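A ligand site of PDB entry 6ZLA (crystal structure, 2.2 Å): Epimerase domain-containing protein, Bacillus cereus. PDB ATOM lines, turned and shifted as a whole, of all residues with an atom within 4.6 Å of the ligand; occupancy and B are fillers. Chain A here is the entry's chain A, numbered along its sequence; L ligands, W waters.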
ATOM      1  N   GLY A   7      28.787 -26.367  17.974  1.00  0.00           N
ATOM      2  CA  GLY A   7      27.865 -25.310  17.530  1.00  0.00           C
ATOM      3  C   GLY A   7      26.418 -25.588  17.899  1.00  0.00           C
ATOM      4  O   GLY A   7      25.515 -25.098  17.197  1.00  0.00           O
ATOM      5  N   ALA A   9      24.335 -24.449  20.214  1.00  0.00           N
ATOM      6  CA  ALA A   9      23.434 -23.316  20.528  1.00  0.00           C
ATOM      7  C   ALA A   9      23.020 -22.578  19.239  1.00  0.00           C
ATOM      8  O   ALA A   9      22.204 -21.700  19.313  1.00  0.00           O
ATOM      9  CB  ALA A   9      24.074 -22.358  21.498  1.00  0.00           C
ATOM     10  N   GLY A  10      23.592 -22.909  18.095  1.00  0.00           N
ATOM     11  CA  GLY A  10      23.259 -22.254  16.813  1.00  0.00           C
ATOM     12  C   GLY A  10      21.926 -22.698  16.250  1.00  0.00           C
ATOM     13  O   GLY A  10      21.243 -23.573  16.814  1.00  0.00           O
ATOM     14  N   PHE A  11      21.603 -22.140  15.089  1.00  0.00           N
ATOM     15  CA  PHE A  11      20.354 -22.411  14.340  1.00  0.00           C
ATOM     16  C   PHE A  11      20.228 -23.923  14.132  1.00  0.00           C
ATOM     17  O   PHE A  11      19.303 -24.520  14.674  1.00  0.00           O
ATOM     18  CB  PHE A  11      20.373 -21.569  13.059  1.00  0.00           C
ATOM     19  CG  PHE A  11      19.397 -21.967  11.962  1.00  0.00           C
ATOM     20  CD1 PHE A  11      18.119 -22.425  12.259  1.00  0.00           C
ATOM     21  CD2 PHE A  11      19.754 -21.806  10.629  1.00  0.00           C
ATOM     22  CE1 PHE A  11      17.216 -22.732  11.254  1.00  0.00           C
ATOM     23  CE2 PHE A  11      18.859 -22.144   9.620  1.00  0.00           C
ATOM     24  CZ  PHE A  11      17.591 -22.596   9.933  1.00  0.00           C
ATOM     25  N   ILE A  12      21.118 -24.536  13.364  1.00  0.00           N
ATOM     26  CA  ILE A  12      20.990 -25.977  12.953  1.00  0.00           C
ATOM     27  C   ILE A  12      21.382 -26.892  14.128  1.00  0.00           C
ATOM     28  O   ILE A  12      20.641 -27.870  14.395  1.00  0.00           O
ATOM     29  CB  ILE A  12      21.781 -26.262  11.664  1.00  0.00           C
ATOM     30  CG1 ILE A  12      21.438 -25.222  10.595  1.00  0.00           C
ATOM     31  CG2 ILE A  12      21.499 -27.680  11.191  1.00  0.00           C
ATOM     32  CD1 ILE A  12      22.165 -25.411   9.270  1.00  0.00           C
ATOM     33  N   GLY A  13      22.448 -26.552  14.840  1.00  0.00           N
ATOM     34  CA  GLY A  13      22.948 -27.388  15.952  1.00  0.00           C
ATOM     35  C   GLY A  13      21.888 -27.559  17.020  1.00  0.00           C
ATOM     36  O   GLY A  13      21.752 -28.693  17.505  1.00  0.00           O
ATOM     37  N   ILE A  31      28.697 -28.244  22.527  1.00  0.00           N
ATOM     38  CA  ILE A  31      29.672 -27.179  22.865  1.00  0.00           C
ATOM     39  C   ILE A  31      29.407 -25.984  21.947  1.00  0.00           C
ATOM     40  O   ILE A  31      29.106 -26.172  20.762  1.00  0.00           O
ATOM     41  CB  ILE A  31      31.123 -27.704  22.795  1.00  0.00           C
ATOM     42  CG1 ILE A  31      32.123 -26.645  23.269  1.00  0.00           C
ATOM     43  CG2 ILE A  31      31.462 -28.200  21.402  1.00  0.00           C
ATOM     44  CD1 ILE A  31      33.467 -27.202  23.643  1.00  0.00           C
ATOM     45  N   ASP A  32      29.415 -24.796  22.512  1.00  0.00           N
ATOM     46  CA  ASP A  32      29.148 -23.521  21.813  1.00  0.00           C
ATOM     47  C   ASP A  32      29.730 -22.400  22.654  1.00  0.00           C
ATOM     48  O   ASP A  32      29.527 -22.400  23.898  1.00  0.00           O
ATOM     49  CB  ASP A  32      27.650 -23.324  21.571  1.00  0.00           C
ATOM     50  CG  ASP A  32      27.412 -22.425  20.380  1.00  0.00           C
ATOM     51  OD1 ASP A  32      27.829 -21.251  20.465  1.00  0.00           O
ATOM     52  OD2 ASP A  32      26.808 -22.912  19.345  1.00  0.00           O
ATOM     53  N   HIS A  33      30.421 -21.478  22.003  1.00  0.00           N
ATOM     54  CA  HIS A  33      31.113 -20.325  22.636  1.00  0.00           C
ATOM     55  C   HIS A  33      30.298 -19.027  22.402  1.00  0.00           C
ATOM     56  O   HIS A  33      30.746 -18.001  22.840  1.00  0.00           O
ATOM     57  CB  HIS A  33      32.549 -20.345  22.069  1.00  0.00           C
ATOM     58  CG  HIS A  33      33.473 -19.330  22.635  1.00  0.00           C
ATOM     59  ND1 HIS A  33      33.485 -19.001  23.985  1.00  0.00           N
ATOM     60  CD2 HIS A  33      34.422 -18.577  22.039  1.00  0.00           C
ATOM     61  CE1 HIS A  33      34.405 -18.071  24.187  1.00  0.00           C
ATOM     62  NE2 HIS A  33      34.994 -17.797  23.012  1.00  0.00           N
ATOM     63  N   PHE A  34      29.172 -19.077  21.697  1.00  0.00           N
ATOM     64  CA  PHE A  34      28.243 -17.910  21.500  1.00  0.00           C
ATOM     65  C   PHE A  34      28.972 -16.790  20.757  1.00  0.00           C
ATOM     66  O   PHE A  34      29.119 -15.678  21.290  1.00  0.00           O
ATOM     67  CB  PHE A  34      27.650 -17.397  22.822  1.00  0.00           C
ATOM     68  CG  PHE A  34      26.577 -18.304  23.384  1.00  0.00           C
ATOM     69  CD1 PHE A  34      26.898 -19.556  23.901  1.00  0.00           C
ATOM     70  CD2 PHE A  34      25.240 -17.944  23.349  1.00  0.00           C
ATOM     71  CE1 PHE A  34      25.912 -20.395  24.405  1.00  0.00           C
ATOM     72  CE2 PHE A  34      24.251 -18.791  23.833  1.00  0.00           C
ATOM     73  CZ  PHE A  34      24.586 -20.014  24.367  1.00  0.00           C
ATOM     74  N   ILE A  35      29.391 -17.083  19.533  1.00  0.00           N
ATOM     75  CA  ILE A  35      30.072 -16.090  18.646  1.00  0.00           C
ATOM     76  C   ILE A  35      29.450 -16.196  17.256  1.00  0.00           C
ATOM     77  O   ILE A  35      28.537 -17.009  17.052  1.00  0.00           O
ATOM     78  CB  ILE A  35      31.597 -16.303  18.628  1.00  0.00           C
ATOM     79  CG1 ILE A  35      32.010 -17.654  18.037  1.00  0.00           C
ATOM     80  CG2 ILE A  35      32.180 -16.085  20.022  1.00  0.00           C
ATOM     81  CD1 ILE A  35      33.530 -17.803  17.794  1.00  0.00           C
ATOM     82  N   PRO A  37      27.483 -14.340  13.832  1.00  0.00           N
ATOM     83  CA  PRO A  37      26.565 -13.244  13.507  1.00  0.00           C
ATOM     84  C   PRO A  37      25.311 -13.122  14.380  1.00  0.00           C
ATOM     85  O   PRO A  37      24.830 -12.041  14.522  1.00  0.00           O
ATOM     86  CB  PRO A  37      26.177 -13.514  12.034  1.00  0.00           C
ATOM     87  CG  PRO A  37      26.391 -15.033  11.864  1.00  0.00           C
ATOM     88  CD  PRO A  37      27.521 -15.393  12.808  1.00  0.00           C
ATOM     89  N   THR A  38      24.816 -14.219  14.966  1.00  0.00           N
ATOM     90  CA  THR A  38      23.661 -14.214  15.898  1.00  0.00           C
ATOM     91  C   THR A  38      24.072 -13.722  17.291  1.00  0.00           C
ATOM     92  O   THR A  38      24.834 -14.381  17.989  1.00  0.00           O
ATOM     93  CB  THR A  38      23.045 -15.610  16.029  1.00  0.00           C
ATOM     94  OG1 THR A  38      22.726 -16.045  14.706  1.00  0.00           O
ATOM     95  CG2 THR A  38      21.794 -15.631  16.884  1.00  0.00           C
ATOM     96  N   LYS A  43      20.431 -15.976  20.910  1.00  0.00           N
ATOM     97  CA  LYS A  43      20.952 -17.371  20.731  1.00  0.00           C
ATOM     98  C   LYS A  43      20.504 -18.223  21.926  1.00  0.00           C
ATOM     99  O   LYS A  43      20.156 -19.379  21.702  1.00  0.00           O
ATOM    100  CB  LYS A  43      22.488 -17.303  20.529  1.00  0.00           C
ATOM    101  CG  LYS A  43      23.222 -18.526  19.970  1.00  0.00           C
ATOM    102  CD  LYS A  43      24.031 -18.230  18.672  1.00  0.00           C
ATOM    103  CE  LYS A  43      25.529 -17.994  18.776  1.00  0.00           C
ATOM    104  NZ  LYS A  43      25.892 -16.674  19.374  1.00  0.00           N
ATOM    105  N   GLU A  61      32.133 -23.129  26.045  1.00  0.00           N
ATOM    106  CA  GLU A  61      33.608 -22.957  25.926  1.00  0.00           C
ATOM    107  C   GLU A  61      33.969 -22.811  24.447  1.00  0.00           C
ATOM    108  O   GLU A  61      33.221 -23.337  23.583  1.00  0.00           O
ATOM    109  CB  GLU A  61      34.382 -24.106  26.577  1.00  0.00           C
ATOM    110  CG  GLU A  61      34.119 -24.237  28.062  1.00  0.00           C
ATOM    111  CD  GLU A  61      34.942 -25.242  28.875  1.00  0.00           C
ATOM    112  OE1 GLU A  61      36.013 -25.712  28.409  1.00  0.00           O
ATOM    113  OE2 GLU A  61      34.504 -25.540  30.013  1.00  0.00           O
ATOM    114  N   ASP A  62      35.047 -22.084  24.180  1.00  0.00           N
ATOM    115  CA  ASP A  62      35.721 -22.087  22.864  1.00  0.00           C
ATOM    116  C   ASP A  62      36.305 -23.488  22.673  1.00  0.00           C
ATOM    117  O   ASP A  62      37.035 -23.930  23.566  1.00  0.00           O
ATOM    118  CB  ASP A  62      36.826 -21.039  22.763  1.00  0.00           C
ATOM    119  CG  ASP A  62      37.249 -20.732  21.330  1.00  0.00           C
ATOM    120  OD1 ASP A  62      37.187 -21.624  20.454  1.00  0.00           O
ATOM    121  OD2 ASP A  62      37.629 -19.593  21.089  1.00  0.00           O
ATOM    122  N   ILE A  63      35.981 -24.144  21.555  1.00  0.00           N
ATOM    123  CA  ILE A  63      36.627 -25.408  21.106  1.00  0.00           C
ATOM    124  C   ILE A  63      38.148 -25.254  21.179  1.00  0.00           C
ATOM    125  O   ILE A  63      38.797 -26.233  21.552  1.00  0.00           O
ATOM    126  CB  ILE A  63      36.150 -25.849  19.697  1.00  0.00           C
ATOM    127  CG1 ILE A  63      34.691 -26.294  19.716  1.00  0.00           C
ATOM    128  CG2 ILE A  63      37.039 -26.959  19.131  1.00  0.00           C
ATOM    129  CD1 ILE A  63      34.012 -26.194  18.365  1.00  0.00           C
ATOM    130  N   LEU A  81      29.420 -28.743  13.564  1.00  0.00           N
ATOM    131  CA  LEU A  81      28.638 -27.634  12.959  1.00  0.00           C
ATOM    132  C   LEU A  81      29.213 -26.268  13.379  1.00  0.00           C
ATOM    133  O   LEU A  81      28.787 -25.273  12.795  1.00  0.00           O
ATOM    134  CB  LEU A  81      27.164 -27.760  13.384  1.00  0.00           C
ATOM    135  CG  LEU A  81      26.349 -28.775  12.573  1.00  0.00           C
ATOM    136  CD1 LEU A  81      26.624 -30.211  13.032  1.00  0.00           C
ATOM    137  CD2 LEU A  81      24.873 -28.454  12.642  1.00  0.00           C
ATOM    138  N   ALA A  82      30.082 -26.182  14.371  1.00  0.00           N
ATOM    139  CA  ALA A  82      30.675 -24.892  14.810  1.00  0.00           C
ATOM    140  C   ALA A  82      31.424 -24.270  13.630  1.00  0.00           C
ATOM    141  O   ALA A  82      32.273 -24.946  13.013  1.00  0.00           O
ATOM    142  CB  ALA A  82      31.583 -25.064  16.006  1.00  0.00           C
ATOM    143  N   ALA A  83      31.112 -23.023  13.322  1.00  0.00           N
ATOM    144  CA  ALA A  83      31.671 -22.265  12.183  1.00  0.00           C
ATOM    145  C   ALA A  83      31.358 -20.800  12.426  1.00  0.00           C
ATOM    146  O   ALA A  83      30.492 -20.506  13.245  1.00  0.00           O
ATOM    147  CB  ALA A  83      31.023 -22.752  10.901  1.00  0.00           C
ATOM    148  N   PRO A  85      29.643 -18.541   9.855  1.00  0.00           N
ATOM    149  CA  PRO A  85      29.013 -18.489   8.531  1.00  0.00           C
ATOM    150  C   PRO A  85      28.683 -17.071   8.040  1.00  0.00           C
ATOM    151  O   PRO A  85      28.752 -16.188   8.852  1.00  0.00           O
ATOM    152  CB  PRO A  85      27.731 -19.280   8.816  1.00  0.00           C
ATOM    153  CG  PRO A  85      27.340 -18.814  10.203  1.00  0.00           C
ATOM    154  CD  PRO A  85      28.656 -18.604  10.934  1.00  0.00           C
ATOM    155  N   ASN A 101      37.965 -20.014  13.192  1.00  0.00           N
ATOM    156  CA  ASN A 101      36.789 -20.820  13.615  1.00  0.00           C
ATOM    157  C   ASN A 101      36.423 -21.844  12.523  1.00  0.00           C
ATOM    158  O   ASN A 101      35.758 -22.815  12.876  1.00  0.00           O
ATOM    159  CB  ASN A 101      35.668 -19.888  14.088  1.00  0.00           C
ATOM    160  CG  ASN A 101      36.102 -19.119  15.316  1.00  0.00           C
ATOM    161  OD1 ASN A 101      36.338 -19.690  16.374  1.00  0.00           O
ATOM    162  ND2 ASN A 101      36.305 -17.824  15.174  1.00  0.00           N
ATOM    163  N   VAL A 105      39.860 -24.487  14.129  1.00  0.00           N
ATOM    164  CA  VAL A 105      38.919 -25.318  14.939  1.00  0.00           C
ATOM    165  C   VAL A 105      38.848 -26.705  14.308  1.00  0.00           C
ATOM    166  O   VAL A 105      38.882 -27.719  15.061  1.00  0.00           O
ATOM    167  CB  VAL A 105      37.520 -24.695  15.025  1.00  0.00           C
ATOM    168  CG1 VAL A 105      36.461 -25.754  15.339  1.00  0.00           C
ATOM    169  CG2 VAL A 105      37.528 -23.565  16.039  1.00  0.00           C
ATOM    170  N   ILE A 124      29.993 -30.742   8.900  1.00  0.00           N
ATOM    171  CA  ILE A 124      28.982 -29.955   8.147  1.00  0.00           C
ATOM    172  C   ILE A 124      29.721 -28.827   7.457  1.00  0.00           C
ATOM    173  O   ILE A 124      30.532 -28.115   8.117  1.00  0.00           O
ATOM    174  CB  ILE A 124      27.819 -29.522   9.061  1.00  0.00           C
ATOM    175  CG1 ILE A 124      26.772 -30.630   9.149  1.00  0.00           C
ATOM    176  CG2 ILE A 124      27.204 -28.235   8.579  1.00  0.00           C
ATOM    177  CD1 ILE A 124      27.321 -31.958   9.565  1.00  0.00           C
ATOM    178  N   SER A 125      29.468 -28.730   6.150  1.00  0.00           N
ATOM    179  CA  SER A 125      30.011 -27.730   5.210  1.00  0.00           C
ATOM    180  C   SER A 125      28.814 -27.041   4.527  1.00  0.00           C
ATOM    181  O   SER A 125      27.689 -27.140   5.019  1.00  0.00           O
ATOM    182  CB  SER A 125      30.953 -28.400   4.207  1.00  0.00           C
ATOM    183  OG  SER A 125      31.660 -27.423   3.424  1.00  0.00           O
ATOM    184  N   THR A 126      29.076 -26.325   3.444  1.00  0.00           N
ATOM    185  CA  THR A 126      28.146 -25.330   2.879  1.00  0.00           C
ATOM    186  C   THR A 126      28.253 -25.371   1.349  1.00  0.00           C
ATOM    187  O   THR A 126      29.358 -25.670   0.844  1.00  0.00           O
ATOM    188  CB  THR A 126      28.482 -23.949   3.445  1.00  0.00           C
ATOM    189  OG1 THR A 126      27.598 -23.017   2.827  1.00  0.00           O
ATOM    190  CG2 THR A 126      29.923 -23.557   3.171  1.00  0.00           C
ATOM    191  N   TYR A 149      33.986 -17.004   3.576  1.00  0.00           N
ATOM    192  CA  TYR A 149      33.237 -18.131   4.172  1.00  0.00           C
ATOM    193  C   TYR A 149      33.497 -19.414   3.363  1.00  0.00           C
ATOM    194  O   TYR A 149      33.970 -20.449   3.933  1.00  0.00           O
ATOM    195  CB  TYR A 149      31.754 -17.755   4.185  1.00  0.00           C
ATOM    196  CG  TYR A 149      30.805 -18.840   4.603  1.00  0.00           C
ATOM    197  CD1 TYR A 149      31.004 -19.551   5.768  1.00  0.00           C
ATOM    198  CD2 TYR A 149      29.651 -19.091   3.873  1.00  0.00           C
ATOM    199  CE1 TYR A 149      30.106 -20.524   6.182  1.00  0.00           C
ATOM    200  CE2 TYR A 149      28.756 -20.058   4.271  1.00  0.00           C
ATOM    201  CZ  TYR A 149      28.973 -20.780   5.429  1.00  0.00           C
ATOM    202  OH  TYR A 149      28.069 -21.722   5.810  1.00  0.00           O
ATOM    203  N   LYS A 153      35.573 -22.666   4.666  1.00  0.00           N
ATOM    204  CA  LYS A 153      34.805 -23.929   4.878  1.00  0.00           C
ATOM    205  C   LYS A 153      35.391 -25.010   3.967  1.00  0.00           C
ATOM    206  O   LYS A 153      35.536 -26.160   4.417  1.00  0.00           O
ATOM    207  CB  LYS A 153      33.296 -23.738   4.657  1.00  0.00           C
ATOM    208  CG  LYS A 153      32.597 -22.820   5.668  1.00  0.00           C
ATOM    209  CD  LYS A 153      32.364 -23.476   7.023  1.00  0.00           C
ATOM    210  CE  LYS A 153      31.497 -24.720   6.939  1.00  0.00           C
ATOM    211  NZ  LYS A 153      31.238 -25.268   8.279  1.00  0.00           N
ATOM    212  N   TYR A 176      25.359 -28.393   3.214  1.00  0.00           N
ATOM    213  CA  TYR A 176      24.000 -27.826   3.372  1.00  0.00           C
ATOM    214  C   TYR A 176      23.860 -26.720   2.323  1.00  0.00           C
ATOM    215  O   TYR A 176      24.814 -25.948   2.117  1.00  0.00           O
ATOM    216  CB  TYR A 176      23.762 -27.252   4.769  1.00  0.00           C
ATOM    217  CG  TYR A 176      23.696 -28.197   5.946  1.00  0.00           C
ATOM    218  CD1 TYR A 176      23.436 -29.556   5.811  1.00  0.00           C
ATOM    219  CD2 TYR A 176      23.904 -27.723   7.237  1.00  0.00           C
ATOM    220  CE1 TYR A 176      23.360 -30.401   6.904  1.00  0.00           C
ATOM    221  CE2 TYR A 176      23.837 -28.553   8.343  1.00  0.00           C
ATOM    222  CZ  TYR A 176      23.556 -29.899   8.192  1.00  0.00           C
ATOM    223  OH  TYR A 176      23.480 -30.687   9.299  1.00  0.00           O
ATOM    224  N   PHE A 177      22.724 -26.676   1.649  1.00  0.00           N
ATOM    225  CA  PHE A 177      22.273 -25.521   0.853  1.00  0.00           C
ATOM    226  C   PHE A 177      21.377 -24.733   1.805  1.00  0.00           C
ATOM    227  O   PHE A 177      21.115 -25.268   2.890  1.00  0.00           O
ATOM    228  CB  PHE A 177      21.606 -25.973  -0.443  1.00  0.00           C
ATOM    229  CG  PHE A 177      22.576 -26.500  -1.472  1.00  0.00           C
ATOM    230  CD1 PHE A 177      23.364 -27.605  -1.186  1.00  0.00           C
ATOM    231  CD2 PHE A 177      22.712 -25.874  -2.715  1.00  0.00           C
ATOM    232  CE1 PHE A 177      24.258 -28.094  -2.132  1.00  0.00           C
ATOM    233  CE2 PHE A 177      23.635 -26.351  -3.634  1.00  0.00           C
ATOM    234  CZ  PHE A 177      24.395 -27.461  -3.354  1.00  0.00           C
ATOM    235  N   THR A 178      20.985 -23.530   1.427  1.00  0.00           N
ATOM    236  CA  THR A 178      20.297 -22.536   2.276  1.00  0.00           C
ATOM    237  C   THR A 178      19.203 -23.211   3.107  1.00  0.00           C
ATOM    238  O   THR A 178      18.242 -23.729   2.489  1.00  0.00           O
ATOM    239  CB  THR A 178      19.656 -21.444   1.425  1.00  0.00           C
ATOM    240  OG1 THR A 178      20.808 -20.898   0.797  1.00  0.00           O
ATOM    241  CG2 THR A 178      18.906 -20.404   2.244  1.00  0.00           C
ATOM    242  N   VAL A 179      19.376 -23.178   4.425  1.00  0.00           N
ATOM    243  CA  VAL A 179      18.434 -23.807   5.404  1.00  0.00           C
ATOM    244  C   VAL A 179      17.621 -22.658   5.994  1.00  0.00           C
ATOM    245  O   VAL A 179      18.234 -21.629   6.338  1.00  0.00           O
ATOM    246  CB  VAL A 179      19.151 -24.617   6.505  1.00  0.00           C
ATOM    247  CG1 VAL A 179      18.163 -25.198   7.519  1.00  0.00           C
ATOM    248  CG2 VAL A 179      20.046 -25.708   5.928  1.00  0.00           C
ATOM    249  N   ARG A 185      19.168 -17.808  11.459  1.00  0.00           N
ATOM    250  CA  ARG A 185      20.097 -16.719  11.891  1.00  0.00           C
ATOM    251  C   ARG A 185      19.543 -15.387  11.389  1.00  0.00           C
ATOM    252  O   ARG A 185      18.942 -15.343  10.325  1.00  0.00           O
ATOM    253  CB  ARG A 185      21.515 -16.851  11.344  1.00  0.00           C
ATOM    254  CG  ARG A 185      22.171 -18.229  11.461  1.00  0.00           C
ATOM    255  CD  ARG A 185      23.657 -18.111  11.270  1.00  0.00           C
ATOM    256  NE  ARG A 185      23.996 -17.436  10.028  1.00  0.00           N
ATOM    257  CZ  ARG A 185      24.289 -18.020   8.877  1.00  0.00           C
ATOM    258  NH1 ARG A 185      24.273 -19.337   8.770  1.00  0.00           N
ATOM    259  NH2 ARG A 185      24.579 -17.283   7.817  1.00  0.00           N
ATOM    260  N   MET A 188      20.311 -13.904   7.831  1.00  0.00           N
ATOM    261  CA  MET A 188      19.865 -14.653   6.639  1.00  0.00           C
ATOM    262  C   MET A 188      18.626 -13.985   6.042  1.00  0.00           C
ATOM    263  O   MET A 188      17.900 -13.260   6.760  1.00  0.00           O
ATOM    264  CB  MET A 188      19.620 -16.123   6.979  1.00  0.00           C
ATOM    265  CG  MET A 188      20.922 -16.859   7.340  1.00  0.00           C
ATOM    266  SD  MET A 188      20.716 -18.618   7.621  1.00  0.00           S
ATOM    267  CE  MET A 188      20.391 -19.129   5.931  1.00  0.00           C
HETATM  268  P1  LIG L   1      25.147 -20.540  13.701  1.00  0.00           P
HETATM  269  O1  LIG L   1      23.730 -20.410  14.174  1.00  0.00           O
HETATM  270  O2  LIG L   1      26.052 -19.375  13.818  1.00  0.00           O
HETATM  271  O3  LIG L   1      25.807 -21.768  14.482  1.00  0.00           O
HETATM  272  C1  LIG L   1      27.227 -21.914  14.553  1.00  0.00           C
HETATM  273  C2  LIG L   1      27.577 -21.959  16.015  1.00  0.00           C
HETATM  274  O4  LIG L   1      28.975 -22.280  16.145  1.00  0.00           O
HETATM  275  C3  LIG L   1      27.342 -20.653  16.786  1.00  0.00           C
HETATM  276  O5  LIG L   1      26.381 -20.842  17.825  1.00  0.00           O
HETATM  277  C4  LIG L   1      28.732 -20.315  17.356  1.00  0.00           C
HETATM  278  O6  LIG L   1      28.626 -19.803  18.668  1.00  0.00           O
HETATM  279  C5  LIG L   1      29.441 -21.659  17.325  1.00  0.00           C
HETATM  280  N1  LIG L   1      30.890 -21.582  17.288  1.00  0.00           N
HETATM  281  C6  LIG L   1      31.641 -20.990  16.307  1.00  0.00           C
HETATM  282  N2  LIG L   1      32.928 -21.040  16.536  1.00  0.00           N
HETATM  283  C7  LIG L   1      33.038 -21.744  17.728  1.00  0.00           C
HETATM  284  C8  LIG L   1      34.165 -22.129  18.496  1.00  0.00           C
HETATM  285  N3  LIG L   1      35.434 -21.827  18.181  1.00  0.00           N
HETATM  286  N4  LIG L   1      33.917 -22.850  19.623  1.00  0.00           N
HETATM  287  C9  LIG L   1      32.641 -23.120  19.943  1.00  0.00           C
HETATM  288  N5  LIG L   1      31.517 -22.784  19.318  1.00  0.00           N
HETATM  289  C10 LIG L   1      31.786 -22.093  18.191  1.00  0.00           C
HETATM  290  O7  LIG L   1      25.192 -21.166  12.224  1.00  0.00           O
HETATM  291  P2  LIG L   1      24.142 -22.131  11.504  1.00  0.00           P
HETATM  292  O8  LIG L   1      23.470 -22.958  12.543  1.00  0.00           O
HETATM  293  O9  LIG L   1      23.362 -21.395  10.461  1.00  0.00           O
HETATM  294  O10 LIG L   1      25.197 -23.052  10.731  1.00  0.00           O
HETATM  295  C11 LIG L   1      25.683 -24.263  11.340  1.00  0.00           C
HETATM  296  C12 LIG L   1      26.642 -24.942  10.404  1.00  0.00           C
HETATM  297  O11 LIG L   1      25.944 -25.229   9.174  1.00  0.00           O
HETATM  298  C13 LIG L   1      27.885 -24.137  10.014  1.00  0.00           C
HETATM  299  O12 LIG L   1      29.007 -24.996   9.900  1.00  0.00           O
HETATM  300  C14 LIG L   1      27.509 -23.546   8.648  1.00  0.00           C
HETATM  301  O13 LIG L   1      28.626 -23.249   7.816  1.00  0.00           O
HETATM  302  C15 LIG L   1      26.683 -24.685   8.082  1.00  0.00           C
HETATM  303  N6  LIG L   1      25.697 -24.225   7.057  1.00  0.00           N
HETATM  304  C16 LIG L   1      24.534 -23.549   7.409  1.00  0.00           C
HETATM  305  C17 LIG L   1      23.696 -23.050   6.411  1.00  0.00           C
HETATM  306  C18 LIG L   1      22.434 -22.283   6.727  1.00  0.00           C
HETATM  307  O14 LIG L   1      21.639 -22.080   5.809  1.00  0.00           O
HETATM  308  N7  LIG L   1      22.236 -21.826   7.970  1.00  0.00           N
HETATM  309  C19 LIG L   1      24.045 -23.235   5.061  1.00  0.00           C
HETATM  310  C20 LIG L   1      25.184 -23.960   4.732  1.00  0.00           C
HETATM  311  C21 LIG L   1      25.918 -24.543   5.742  1.00  0.00           C
HETATM  312  O   HOH W   1      22.344 -18.532  15.232  1.00  0.00           O
HETATM  313  O   HOH W   2      28.634 -18.560  14.351  1.00  0.00           O
HETATM  314  O   HOH W   3      25.809 -20.503   6.138  1.00  0.00           O
HETATM  315  O   HOH W   4      24.538 -24.696  14.599  1.00  0.00           O
HETATM  316  O   HOH W   5      26.202 -17.318  15.317  1.00  0.00           O
HETATM  317  O   HOH W   6      31.540 -26.939  10.669  1.00  0.00           O
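An oxygen (O6) of the ligand sits at hydrogen-bond distance from the side-chain carboxylate (OD1) of Asp 32. OH of Tyr 149 lies within hydrogen-bond range of O13 of the ligand, at 2.6 Å. The side-chain amino group of Lys 153 is in hydrogen-bond range of an oxygen (O12) of the ligand, at 2.8 Å. NH1 of Arg 185 is in salt-bridge range of O9 of the ligand. The backbone NH (N) of Val 179 lies within hydrogen-bond range of an oxygen (O14) of the ligand (2.9 Å). A nitrogen (N3) of the ligand is in hydrogen-bond range of the side-chain carboxylate (OD1) of Asp 62 (2.9 Å). The backbone NH (N) of Phe 11 lies within hydrogen-bond range of an oxygen (O1) of the ligand, 2.9 Å away. An oxygen (O12) of the ligand lies within hydrogen-bond range of the backbone carbonyl oxygen of Leu 81 (2.9 Å). OD1 of Asn 101 is in hydrogen-bond range of N3 of the ligand. The backbone NH (N) of Ile 12 is in hydrogen-bond range of an oxygen (O8) of the ligand (2.9 Å). An oxygen (O6) of the ligand sits at hydrogen-bond distance from the backbone NH (N) of Ile 35 (3.0 Å). An oxygen (O6) of the ligand is in hydrogen-bond range of the backbone carbonyl oxygen of Ile 35 (3.2 Å). N4 of the ligand lies within hydrogen-bond range of N of Ile 63 (3.1 Å). O6 of the ligand lies within hydrogen-bond range of N of Phe 34. The backbone NH of His 33 lies within hydrogen-bond range of a nitrogen (N5) of the ligand (3.2 Å). The side-chain sulfur (SD) of Met 188 lies within hydrogen-bond range of a nitrogen (N7) of the ligand, at 3.6 Å. N of Gly 10 sits at hydrogen-bond distance from O5 of the ligand (3.5 Å).
OD1 of Asp 32 is in hydrogen-bond range of N of Phe 34 (2.8 Å). OD2 of Asp 32 lies within hydrogen-bond range of N of Gly 10, at 3.5 Å. O of Asp 32 is in hydrogen-bond range of N of Glu 61 (3.5 Å). The backbone NH of Ala 9 lies within hydrogen-bond range of the side-chain carboxylate of Asp 32, 3.0 Å away. OH of Tyr 149 sits close to OG1 of Thr 126, at 3.3 Å. NZ of Lys 153 lies within hydrogen-bond range of O of Ile 124. A ring nitrogen (ND1) of His 33 lies within hydrogen-bond range of the backbone NH (N) of Asp 62. The backbone NH (N) of Gly 7 lies within hydrogen-bond range of the backbone carbonyl oxygen (O) of Ile 31 (2.8 Å).
Merely in contact with the ligand: Gly 7, Lys 43, Glu 61, Ala 82, Ala 83, Pro 85, Val 105, Ile 124, Ser 125, Thr 126, Tyr 176 and Thr 178. Hydrophobic or aromatic side chains within 4 Å of the ligand: Phe 11, Ile 12, His 33, Ile 35, Ile 63, Ala 82, Ala 83, Pro 85, Val 105, Ile 124, Tyr 149, Tyr 176, Val 179 and Met 188.
Water W5 lies within hydrogen-bond range of O2 of the ligand (2.5 Å), O of Ile 35 (2.9 Å) and N of Thr 38 (3.4 Å). Water W1 bridges O1 of the ligand (2.6 Å) and OG1 of Thr 38 (2.6 Å). Water W2 lies within hydrogen-bond range of O2 of the ligand (2.8 Å), O of Ala 83 (2.9 Å) and O of Ile 35 (3.1 Å). Water W4 lies within hydrogen-bond range of O of Gly 7 (2.8 Å), N of Gly 13 (2.8 Å) and O8 of the ligand (2.9 Å). Water W6 lies within hydrogen-bond range of NZ of Lys 153, O of Ile 124, O of Ala 82 and O12 of the ligand. Water W3 bridges OH of Tyr 149 and NH1 of Arg 185.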
